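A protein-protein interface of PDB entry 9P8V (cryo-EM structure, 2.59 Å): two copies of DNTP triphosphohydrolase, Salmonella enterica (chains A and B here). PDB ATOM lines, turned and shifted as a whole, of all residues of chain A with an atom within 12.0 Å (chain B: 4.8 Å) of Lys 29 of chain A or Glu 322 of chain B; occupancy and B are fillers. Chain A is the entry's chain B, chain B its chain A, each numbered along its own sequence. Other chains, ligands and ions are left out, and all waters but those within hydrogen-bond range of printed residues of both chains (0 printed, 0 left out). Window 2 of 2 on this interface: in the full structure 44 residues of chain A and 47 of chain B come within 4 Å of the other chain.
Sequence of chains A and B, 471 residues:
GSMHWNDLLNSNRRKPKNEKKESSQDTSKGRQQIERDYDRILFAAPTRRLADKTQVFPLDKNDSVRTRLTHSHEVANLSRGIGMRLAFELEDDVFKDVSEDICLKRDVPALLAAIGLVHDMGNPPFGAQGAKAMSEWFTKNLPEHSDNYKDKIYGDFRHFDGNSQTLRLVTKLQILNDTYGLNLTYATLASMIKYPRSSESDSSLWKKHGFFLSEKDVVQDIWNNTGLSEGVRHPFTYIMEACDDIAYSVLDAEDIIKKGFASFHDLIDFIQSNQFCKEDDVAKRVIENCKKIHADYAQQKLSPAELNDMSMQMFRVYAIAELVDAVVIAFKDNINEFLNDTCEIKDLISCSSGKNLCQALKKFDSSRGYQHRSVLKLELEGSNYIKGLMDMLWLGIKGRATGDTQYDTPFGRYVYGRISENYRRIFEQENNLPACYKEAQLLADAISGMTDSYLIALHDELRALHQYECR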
ATOM      1  N   ARG A  13     -29.751  26.957  10.239  1.00  0.00           N
ATOM      2  CA  ARG A  13     -28.404  27.245   9.777  1.00  0.00           C
ATOM      3  C   ARG A  13     -28.330  28.672   9.254  1.00  0.00           C
ATOM      4  O   ARG A  13     -29.339  29.271   8.872  1.00  0.00           O
ATOM      5  CB  ARG A  13     -27.972  26.254   8.691  1.00  0.00           C
ATOM      6  CG  ARG A  13     -28.349  24.816   8.999  1.00  0.00           C
ATOM      7  CD  ARG A  13     -27.563  23.835   8.150  1.00  0.00           C
ATOM      8  NE  ARG A  13     -27.784  22.459   8.576  1.00  0.00           N
ATOM      9  CZ  ARG A  13     -26.895  21.729   9.235  1.00  0.00           C
ATOM     10  NH1 ARG A  13     -25.709  22.213   9.562  1.00  0.00           N
ATOM     11  NH2 ARG A  13     -27.205  20.481   9.574  1.00  0.00           N
ATOM     12  N   THR A  27     -30.110  14.441   0.321  1.00  0.00           N
ATOM     13  CA  THR A  27     -29.486  14.123   1.599  1.00  0.00           C
ATOM     14  C   THR A  27     -30.472  14.302   2.747  1.00  0.00           C
ATOM     15  O   THR A  27     -31.683  14.351   2.530  1.00  0.00           O
ATOM     16  CB  THR A  27     -28.247  14.999   1.856  1.00  0.00           C
ATOM     17  OG1 THR A  27     -28.614  16.382   1.782  1.00  0.00           O
ATOM     18  CG2 THR A  27     -27.169  14.709   0.824  1.00  0.00           C
ATOM     19  N   SER A  28     -29.938  14.402   3.967  1.00  0.00           N
ATOM     20  CA  SER A  28     -30.744  14.574   5.178  1.00  0.00           C
ATOM     21  C   SER A  28     -31.786  13.466   5.314  1.00  0.00           C
ATOM     22  O   SER A  28     -32.926  13.703   5.717  1.00  0.00           O
ATOM     23  CB  SER A  28     -31.411  15.951   5.208  1.00  0.00           C
ATOM     24  OG  SER A  28     -32.494  16.017   4.296  1.00  0.00           O
ATOM     25  N   LYS A  29     -31.388  12.241   4.976  1.00  0.00           N
ATOM     26  CA  LYS A  29     -32.291  11.093   4.991  1.00  0.00           C
ATOM     27  C   LYS A  29     -32.246  10.458   6.376  1.00  0.00           C
ATOM     28  O   LYS A  29     -31.362   9.653   6.675  1.00  0.00           O
ATOM     29  CB  LYS A  29     -31.907  10.097   3.903  1.00  0.00           C
ATOM     30  CG  LYS A  29     -31.657  10.737   2.547  1.00  0.00           C
ATOM     31  CD  LYS A  29     -30.873   9.812   1.630  1.00  0.00           C
ATOM     32  CE  LYS A  29     -30.731  10.408   0.239  1.00  0.00           C
ATOM     33  NZ  LYS A  29     -30.125   9.443  -0.720  1.00  0.00           N
ATOM     34  N   GLY A  30     -33.205  10.822   7.224  1.00  0.00           N
ATOM     35  CA  GLY A  30     -33.304  10.246   8.548  1.00  0.00           C
ATOM     36  C   GLY A  30     -32.302  10.759   9.557  1.00  0.00           C
ATOM     37  O   GLY A  30     -32.139  10.136  10.611  1.00  0.00           O
ATOM     38  N   ARG A  31     -31.629  11.870   9.274  1.00  0.00           N
ATOM     39  CA  ARG A  31     -30.623  12.433  10.163  1.00  0.00           C
ATOM     40  C   ARG A  31     -31.045  13.833  10.584  1.00  0.00           C
ATOM     41  O   ARG A  31     -31.460  14.638   9.744  1.00  0.00           O
ATOM     42  CB  ARG A  31     -29.251  12.479   9.486  1.00  0.00           C
ATOM     43  CG  ARG A  31     -28.921  11.246   8.667  1.00  0.00           C
ATOM     44  CD  ARG A  31     -27.505  10.769   8.939  1.00  0.00           C
ATOM     45  NE  ARG A  31     -26.526  11.835   8.767  1.00  0.00           N
ATOM     46  CZ  ARG A  31     -26.057  12.238   7.595  1.00  0.00           C
ATOM     47  NH1 ARG A  31     -26.460  11.687   6.461  1.00  0.00           N
ATOM     48  NH2 ARG A  31     -25.158  13.219   7.558  1.00  0.00           N
ATOM     49  N   GLN A  32     -30.938  14.116  11.878  1.00  0.00           N
ATOM     50  CA  GLN A  32     -31.204  15.458  12.368  1.00  0.00           C
ATOM     51  C   GLN A  32     -30.094  16.411  11.930  1.00  0.00           C
ATOM     52  O   GLN A  32     -28.974  16.001  11.612  1.00  0.00           O
ATOM     53  CB  GLN A  32     -31.328  15.459  13.892  1.00  0.00           C
ATOM     54  CG  GLN A  32     -32.138  14.302  14.449  1.00  0.00           C
ATOM     55  CD  GLN A  32     -33.596  14.365  14.041  1.00  0.00           C
ATOM     56  OE1 GLN A  32     -34.313  15.297  14.404  1.00  0.00           O
ATOM     57  NE2 GLN A  32     -34.041  13.372  13.280  1.00  0.00           N
ATOM     58  N   GLN A  33     -30.426  17.704  11.907  1.00  0.00           N
ATOM     59  CA  GLN A  33     -29.455  18.708  11.485  1.00  0.00           C
ATOM     60  C   GLN A  33     -28.251  18.736  12.416  1.00  0.00           C
ATOM     61  O   GLN A  33     -27.101  18.816  11.961  1.00  0.00           O
ATOM     62  CB  GLN A  33     -30.121  20.082  11.431  1.00  0.00           C
ATOM     63  CG  GLN A  33     -31.423  20.110  10.652  1.00  0.00           C
ATOM     64  CD  GLN A  33     -31.214  20.001   9.157  1.00  0.00           C
ATOM     65  OE1 GLN A  33     -30.107  20.201   8.657  1.00  0.00           O
ATOM     66  NE2 GLN A  33     -32.279  19.681   8.432  1.00  0.00           N
ATOM     67  N   ILE A  34     -28.494  18.663  13.724  1.00  0.00           N
ATOM     68  CA  ILE A  34     -27.395  18.672  14.683  1.00  0.00           C
ATOM     69  C   ILE A  34     -26.539  17.422  14.524  1.00  0.00           C
ATOM     70  O   ILE A  34     -25.314  17.468  14.687  1.00  0.00           O
ATOM     71  CB  ILE A  34     -27.944  18.812  16.113  1.00  0.00           C
ATOM     72  CG1 ILE A  34     -28.898  20.004  16.198  1.00  0.00           C
ATOM     73  CG2 ILE A  34     -26.809  18.982  17.089  1.00  0.00           C
ATOM     74  CD1 ILE A  34     -29.222  20.435  17.610  1.00  0.00           C
ATOM     75  N   GLU A  35     -27.167  16.287  14.209  1.00  0.00           N
ATOM     76  CA  GLU A  35     -26.403  15.079  13.917  1.00  0.00           C
ATOM     77  C   GLU A  35     -25.536  15.266  12.680  1.00  0.00           C
ATOM     78  O   GLU A  35     -24.383  14.821  12.646  1.00  0.00           O
ATOM     79  CB  GLU A  35     -27.346  13.891  13.736  1.00  0.00           C
ATOM     80  CG  GLU A  35     -27.999  13.412  15.018  1.00  0.00           C
ATOM     81  CD  GLU A  35     -28.847  12.173  14.809  1.00  0.00           C
ATOM     82  OE1 GLU A  35     -28.921  11.691  13.660  1.00  0.00           O
ATOM     83  OE2 GLU A  35     -29.439  11.681  15.792  1.00  0.00           O
ATOM     84  N   ARG A  36     -26.077  15.919  11.649  1.00  0.00           N
ATOM     85  CA  ARG A  36     -25.301  16.191  10.445  1.00  0.00           C
ATOM     86  C   ARG A  36     -24.155  17.158  10.705  1.00  0.00           C
ATOM     87  O   ARG A  36     -23.151  17.118   9.984  1.00  0.00           O
ATOM     88  CB  ARG A  36     -26.212  16.740   9.349  1.00  0.00           C
ATOM     89  CG  ARG A  36     -25.718  16.474   7.939  1.00  0.00           C
ATOM     90  CD  ARG A  36     -26.767  16.862   6.915  1.00  0.00           C
ATOM     91  NE  ARG A  36     -28.114  16.633   7.423  1.00  0.00           N
ATOM     92  CZ  ARG A  36     -29.065  17.556   7.466  1.00  0.00           C
ATOM     93  NH1 ARG A  36     -28.857  18.785   7.022  1.00  0.00           N
ATOM     94  NH2 ARG A  36     -30.253  17.239   7.972  1.00  0.00           N
ATOM     95  N   ASP A  37     -24.283  18.026  11.711  1.00  0.00           N
ATOM     96  CA  ASP A  37     -23.164  18.889  12.079  1.00  0.00           C
ATOM     97  C   ASP A  37     -21.958  18.068  12.515  1.00  0.00           C
ATOM     98  O   ASP A  37     -20.814  18.410  12.188  1.00  0.00           O
ATOM     99  CB  ASP A  37     -23.579  19.852  13.190  1.00  0.00           C
ATOM    100  CG  ASP A  37     -24.378  21.024  12.674  1.00  0.00           C
ATOM    101  OD1 ASP A  37     -24.699  21.043  11.467  1.00  0.00           O
ATOM    102  OD2 ASP A  37     -24.679  21.933  13.473  1.00  0.00           O
ATOM    103  N   ASP A  39     -21.174  15.067  11.468  1.00  0.00           N
ATOM    104  CA  ASP A  39     -20.576  14.519  10.254  1.00  0.00           C
ATOM    105  C   ASP A  39     -19.769  15.577   9.512  1.00  0.00           C
ATOM    106  O   ASP A  39     -18.663  15.301   9.031  1.00  0.00           O
ATOM    107  CB  ASP A  39     -21.661  13.938   9.350  1.00  0.00           C
ATOM    108  CG  ASP A  39     -22.571  12.973  10.082  1.00  0.00           C
ATOM    109  OD1 ASP A  39     -22.366  12.767  11.296  1.00  0.00           O
ATOM    110  OD2 ASP A  39     -23.488  12.417   9.443  1.00  0.00           O
ATOM    111  N   ARG A  40     -20.305  16.796   9.413  1.00  0.00           N
ATOM    112  CA  ARG A  40     -19.579  17.871   8.743  1.00  0.00           C
ATOM    113  C   ARG A  40     -18.255  18.152   9.443  1.00  0.00           C
ATOM    114  O   ARG A  40     -17.224  18.345   8.790  1.00  0.00           O
ATOM    115  CB  ARG A  40     -20.430  19.140   8.693  1.00  0.00           C
ATOM    116  CG  ARG A  40     -21.677  19.047   7.835  1.00  0.00           C
ATOM    117  CD  ARG A  40     -22.791  19.900   8.423  1.00  0.00           C
ATOM    118  NE  ARG A  40     -23.980  19.927   7.580  1.00  0.00           N
ATOM    119  CZ  ARG A  40     -24.090  20.628   6.460  1.00  0.00           C
ATOM    120  NH1 ARG A  40     -23.102  21.388   6.019  1.00  0.00           N
ATOM    121  NH2 ARG A  40     -25.224  20.569   5.768  1.00  0.00           N
ATOM    122  N   PHE A  43     -15.751  14.995   8.976  1.00  0.00           N
ATOM    123  CA  PHE A  43     -15.202  14.848   7.634  1.00  0.00           C
ATOM    124  C   PHE A  43     -14.397  16.061   7.184  1.00  0.00           C
ATOM    125  O   PHE A  43     -13.820  16.027   6.092  1.00  0.00           O
ATOM    126  CB  PHE A  43     -16.323  14.565   6.631  1.00  0.00           C
ATOM    127  CG  PHE A  43     -16.799  13.141   6.646  1.00  0.00           C
ATOM    128  CD1 PHE A  43     -16.164  12.180   5.879  1.00  0.00           C
ATOM    129  CD2 PHE A  43     -17.879  12.762   7.424  1.00  0.00           C
ATOM    130  CE1 PHE A  43     -16.596  10.869   5.889  1.00  0.00           C
ATOM    131  CE2 PHE A  43     -18.316  11.453   7.437  1.00  0.00           C
ATOM    132  CZ  PHE A  43     -17.674  10.505   6.668  1.00  0.00           C
ATOM    133  N   ARG A 106     -31.772  12.516  20.537  1.00  0.00           N
ATOM    134  CA  ARG A 106     -30.881  12.513  19.387  1.00  0.00           C
ATOM    135  C   ARG A 106     -30.085  13.797  19.227  1.00  0.00           C
ATOM    136  O   ARG A 106     -28.993  13.761  18.658  1.00  0.00           O
ATOM    137  CB  ARG A 106     -31.673  12.267  18.097  1.00  0.00           C
ATOM    138  CG  ARG A 106     -32.369  10.923  18.039  1.00  0.00           C
ATOM    139  CD  ARG A 106     -32.988  10.686  16.674  1.00  0.00           C
ATOM    140  NE  ARG A 106     -31.979  10.586  15.628  1.00  0.00           N
ATOM    141  CZ  ARG A 106     -32.223  10.185  14.387  1.00  0.00           C
ATOM    142  NH1 ARG A 106     -33.439   9.837  14.002  1.00  0.00           N
ATOM    143  NH2 ARG A 106     -31.223  10.133  13.514  1.00  0.00           N
ATOM    144  N   ARG B  85     -30.755   5.519  12.756  1.00  0.00           N
ATOM    145  CA  ARG B  85     -31.857   5.269  11.834  1.00  0.00           C
ATOM    146  C   ARG B  85     -32.572   3.953  12.108  1.00  0.00           C
ATOM    147  O   ARG B  85     -33.710   3.783  11.664  1.00  0.00           O
ATOM    148  CB  ARG B  85     -31.363   5.279  10.387  1.00  0.00           C
ATOM    149  CG  ARG B  85     -30.970   6.647   9.867  1.00  0.00           C
ATOM    150  CD  ARG B  85     -30.673   6.582   8.382  1.00  0.00           C
ATOM    151  NE  ARG B  85     -31.592   5.681   7.696  1.00  0.00           N
ATOM    152  CZ  ARG B  85     -32.412   6.043   6.721  1.00  0.00           C
ATOM    153  NH1 ARG B  85     -32.458   7.290   6.283  1.00  0.00           N
ATOM    154  NH2 ARG B  85     -33.209   5.132   6.171  1.00  0.00           N
ATOM    155  N   VAL B 282     -28.724   4.580  -8.726  1.00  0.00           N
ATOM    156  CA  VAL B 282     -28.000   5.290  -7.674  1.00  0.00           C
ATOM    157  C   VAL B 282     -26.799   6.025  -8.256  1.00  0.00           C
ATOM    158  O   VAL B 282     -26.552   7.196  -7.939  1.00  0.00           O
ATOM    159  CB  VAL B 282     -27.578   4.311  -6.562  1.00  0.00           C
ATOM    160  CG1 VAL B 282     -26.771   5.035  -5.496  1.00  0.00           C
ATOM    161  CG2 VAL B 282     -28.798   3.642  -5.953  1.00  0.00           C
ATOM    162  N   ARG B 285     -27.997   9.059 -10.222  1.00  0.00           N
ATOM    163  CA  ARG B 285     -28.384  10.166  -9.354  1.00  0.00           C
ATOM    164  C   ARG B 285     -27.163  10.866  -8.774  1.00  0.00           C
ATOM    165  O   ARG B 285     -27.103  12.104  -8.740  1.00  0.00           O
ATOM    166  CB  ARG B 285     -29.292   9.662  -8.233  1.00  0.00           C
ATOM    167  CG  ARG B 285     -30.698   9.310  -8.678  1.00  0.00           C
ATOM    168  CD  ARG B 285     -31.622   9.152  -7.484  1.00  0.00           C
ATOM    169  NE  ARG B 285     -31.023   8.331  -6.439  1.00  0.00           N
ATOM    170  CZ  ARG B 285     -31.460   7.129  -6.091  1.00  0.00           C
ATOM    171  NH1 ARG B 285     -32.499   6.571  -6.690  1.00  0.00           N
ATOM    172  NH2 ARG B 285     -30.838   6.470  -5.117  1.00  0.00           N
ATOM    173  N   VAL B 286     -26.180  10.091  -8.315  1.00  0.00           N
ATOM    174  CA  VAL B 286     -24.974  10.685  -7.744  1.00  0.00           C
ATOM    175  C   VAL B 286     -24.239  11.506  -8.795  1.00  0.00           C
ATOM    176  O   VAL B 286     -23.808  12.636  -8.532  1.00  0.00           O
ATOM    177  CB  VAL B 286     -24.070   9.593  -7.143  1.00  0.00           C
ATOM    178  CG1 VAL B 286     -22.719  10.174  -6.764  1.00  0.00           C
ATOM    179  CG2 VAL B 286     -24.736   8.968  -5.931  1.00  0.00           C
ATOM    180  N   TYR B 318     -22.899  13.201  -1.422  1.00  0.00           N
ATOM    181  CA  TYR B 318     -23.963  12.527  -2.158  1.00  0.00           C
ATOM    182  C   TYR B 318     -23.778  11.014  -2.154  1.00  0.00           C
ATOM    183  O   TYR B 318     -24.733  10.270  -1.896  1.00  0.00           O
ATOM    184  CB  TYR B 318     -24.022  13.056  -3.589  1.00  0.00           C
ATOM    185  CG  TYR B 318     -24.462  14.498  -3.685  1.00  0.00           C
ATOM    186  CD1 TYR B 318     -25.470  14.991  -2.870  1.00  0.00           C
ATOM    187  CD2 TYR B 318     -23.867  15.367  -4.586  1.00  0.00           C
ATOM    188  CE1 TYR B 318     -25.875  16.308  -2.953  1.00  0.00           C
ATOM    189  CE2 TYR B 318     -24.264  16.686  -4.676  1.00  0.00           C
ATOM    190  CZ  TYR B 318     -25.268  17.150  -3.857  1.00  0.00           C
ATOM    191  OH  TYR B 318     -25.668  18.464  -3.943  1.00  0.00           O
ATOM    192  N   ALA B 319     -22.563  10.540  -2.441  1.00  0.00           N
ATOM    193  CA  ALA B 319     -22.320   9.104  -2.501  1.00  0.00           C
ATOM    194  C   ALA B 319     -22.516   8.454  -1.140  1.00  0.00           C
ATOM    195  O   ALA B 319     -23.120   7.382  -1.040  1.00  0.00           O
ATOM    196  CB  ALA B 319     -20.913   8.835  -3.032  1.00  0.00           C
ATOM    197  N   ILE B 320     -22.013   9.086  -0.075  1.00  0.00           N
ATOM    198  CA  ILE B 320     -22.181   8.527   1.261  1.00  0.00           C
ATOM    199  C   ILE B 320     -23.655   8.459   1.626  1.00  0.00           C
ATOM    200  O   ILE B 320     -24.132   7.435   2.129  1.00  0.00           O
ATOM    201  CB  ILE B 320     -21.378   9.344   2.291  1.00  0.00           C
ATOM    202  CG1 ILE B 320     -19.876   9.127   2.095  1.00  0.00           C
ATOM    203  CG2 ILE B 320     -21.795   8.980   3.707  1.00  0.00           C
ATOM    204  CD1 ILE B 320     -19.358   7.839   2.682  1.00  0.00           C
ATOM    205  N   ALA B 321     -24.407   9.534   1.364  1.00  0.00           N
ATOM    206  CA  ALA B 321     -25.827   9.521   1.695  1.00  0.00           C
ATOM    207  C   ALA B 321     -26.563   8.425   0.933  1.00  0.00           C
ATOM    208  O   ALA B 321     -27.331   7.655   1.524  1.00  0.00           O
ATOM    209  CB  ALA B 321     -26.446  10.887   1.405  1.00  0.00           C
ATOM    210  N   GLU B 322     -26.325   8.327  -0.379  1.00  0.00           N
ATOM    211  CA  GLU B 322     -27.032   7.337  -1.184  1.00  0.00           C
ATOM    212  C   GLU B 322     -26.670   5.917  -0.768  1.00  0.00           C
ATOM    213  O   GLU B 322     -27.554   5.062  -0.629  1.00  0.00           O
ATOM    214  CB  GLU B 322     -26.729   7.556  -2.665  1.00  0.00           C
ATOM    215  CG  GLU B 322     -27.385   8.794  -3.254  1.00  0.00           C
ATOM    216  CD  GLU B 322     -28.833   8.562  -3.642  1.00  0.00           C
ATOM    217  OE1 GLU B 322     -29.312   7.417  -3.506  1.00  0.00           O
ATOM    218  OE2 GLU B 322     -29.491   9.526  -4.084  1.00  0.00           O
ATOM    219  N   LEU B 323     -25.380   5.644  -0.559  1.00  0.00           N
ATOM    220  CA  LEU B 323     -24.958   4.302  -0.178  1.00  0.00           C
ATOM    221  C   LEU B 323     -25.483   3.924   1.201  1.00  0.00           C
ATOM    222  O   LEU B 323     -25.911   2.784   1.412  1.00  0.00           O
ATOM    223  CB  LEU B 323     -23.435   4.202  -0.223  1.00  0.00           C
ATOM    224  CG  LEU B 323     -22.800   4.218  -1.615  1.00  0.00           C
ATOM    225  CD1 LEU B 323     -21.287   4.281  -1.512  1.00  0.00           C
ATOM    226  CD2 LEU B 323     -23.235   3.003  -2.411  1.00  0.00           C
ATOM    227  N   VAL B 324     -25.462   4.861   2.152  1.00  0.00           N
ATOM    228  CA  VAL B 324     -25.975   4.571   3.487  1.00  0.00           C
ATOM    229  C   VAL B 324     -27.469   4.288   3.432  1.00  0.00           C
ATOM    230  O   VAL B 324     -27.960   3.350   4.072  1.00  0.00           O
ATOM    231  CB  VAL B 324     -25.645   5.730   4.447  1.00  0.00           C
ATOM    232  CG1 VAL B 324     -26.562   5.702   5.658  1.00  0.00           C
ATOM    233  CG2 VAL B 324     -24.192   5.657   4.878  1.00  0.00           C
ATOM    234  N   ASP B 325     -28.216   5.085   2.663  1.00  0.00           N
ATOM    235  CA  ASP B 325     -29.650   4.840   2.543  1.00  0.00           C
ATOM    236  C   ASP B 325     -29.926   3.484   1.906  1.00  0.00           C
ATOM    237  O   ASP B 325     -30.809   2.745   2.360  1.00  0.00           O
ATOM    238  CB  ASP B 325     -30.308   5.959   1.736  1.00  0.00           C
ATOM    239  CG  ASP B 325     -31.805   6.030   1.956  1.00  0.00           C
ATOM    240  OD1 ASP B 325     -32.509   5.067   1.588  1.00  0.00           O
ATOM    241  OD2 ASP B 325     -32.279   7.047   2.505  1.00  0.00           O
ATOM    242  N   ALA B 326     -29.177   3.137   0.856  1.00  0.00           N
ATOM    243  CA  ALA B 326     -29.366   1.843   0.211  1.00  0.00           C
ATOM    244  C   ALA B 326     -29.051   0.698   1.164  1.00  0.00           C
ATOM    245  O   ALA B 326     -29.767  -0.311   1.192  1.00  0.00           O
ATOM    246  CB  ALA B 326     -28.499   1.753  -1.044  1.00  0.00           C
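The side-chain carboxylate of Asp 325 of chain B lies within salt-bridge range of the guanidinium group of Arg 85 of chain B (3.8 Å). The guanidinium group (NH2) of Arg 285 of chain B is in salt-bridge range of the side-chain carboxylate (OE1) of Glu 322 of chain B (2.4 Å). The backbone carbonyl oxygen (O) of Gly 30 of chain A is in hydrogen-bond range of the guanidinium group (NH2) of Arg 106 of chain A, at 3.0 Å.
No position is printed for both chains. Of the 5 pairs that touch across the chains among the printed residues, none has its exchanged pair printed and touching as well.
Printed residues of chain B within 4 Å of Thr 27 of chain A: Ala 321. Printed residues of chain B within 4 Å of Lys 29 of chain A: Arg 85 (2.6 Å), Glu 322 (3.3 Å) and Asp 325 (3.2 Å). Of the printed residues of chain B, Gly 30 of chain A touches Arg 85. Printed residues of chain A within 4 Å of Arg 85 of chain B: Lys 29 and Gly 30. No residue of chain A comes within 4 Å of Val 282 of chain B. No residue of chain A comes within 4 Å of Arg 285 of chain B. No residue of chain A comes within 4 Å of Ala 319 of chain B. No residue of chain A comes within 4 Å of Leu 323 of chain B. No residue of chain A comes within 4 Å of Val 324 of chain B. No residue of chain A comes within 4 Å of Ala 326 of chain B. The nearest printed residue of chain B that does not touch Gly 30 of chain A is Asp 325 of chain B (6.1 Å).
Of the 16 printed residues of chain A, 3 touch a printed residue of chain B. Printed residues of chain A that touch a printed residue of chain B: Thr 27, Lys 29 and Gly 30. Among the printed residues, Asp or Glu carboxylates within 4 Å of a Lys or Arg side-chain nitrogen of the other chain: Lys 29 of chain A with Glu 322 of chain B (3.4 Å).
Thr 27 of chain A touches Ala 321 of chain B (CG2 to CB, 3.9 Å). Lys 29 of chain A touches Asp 325 of chain B. Arg 85 of chain B touches Gly 30 of chain A.
The guanidinium group (NH1) of Arg 85 of chain B sits at hydrogen-bond distance from the backbone carbonyl oxygen (O) of Lys 29 of chain A (2.6 Å). OE2 of Glu 322 of chain B is in salt-bridge range of NZ of Lys 29 of chain A (3.4 Å).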
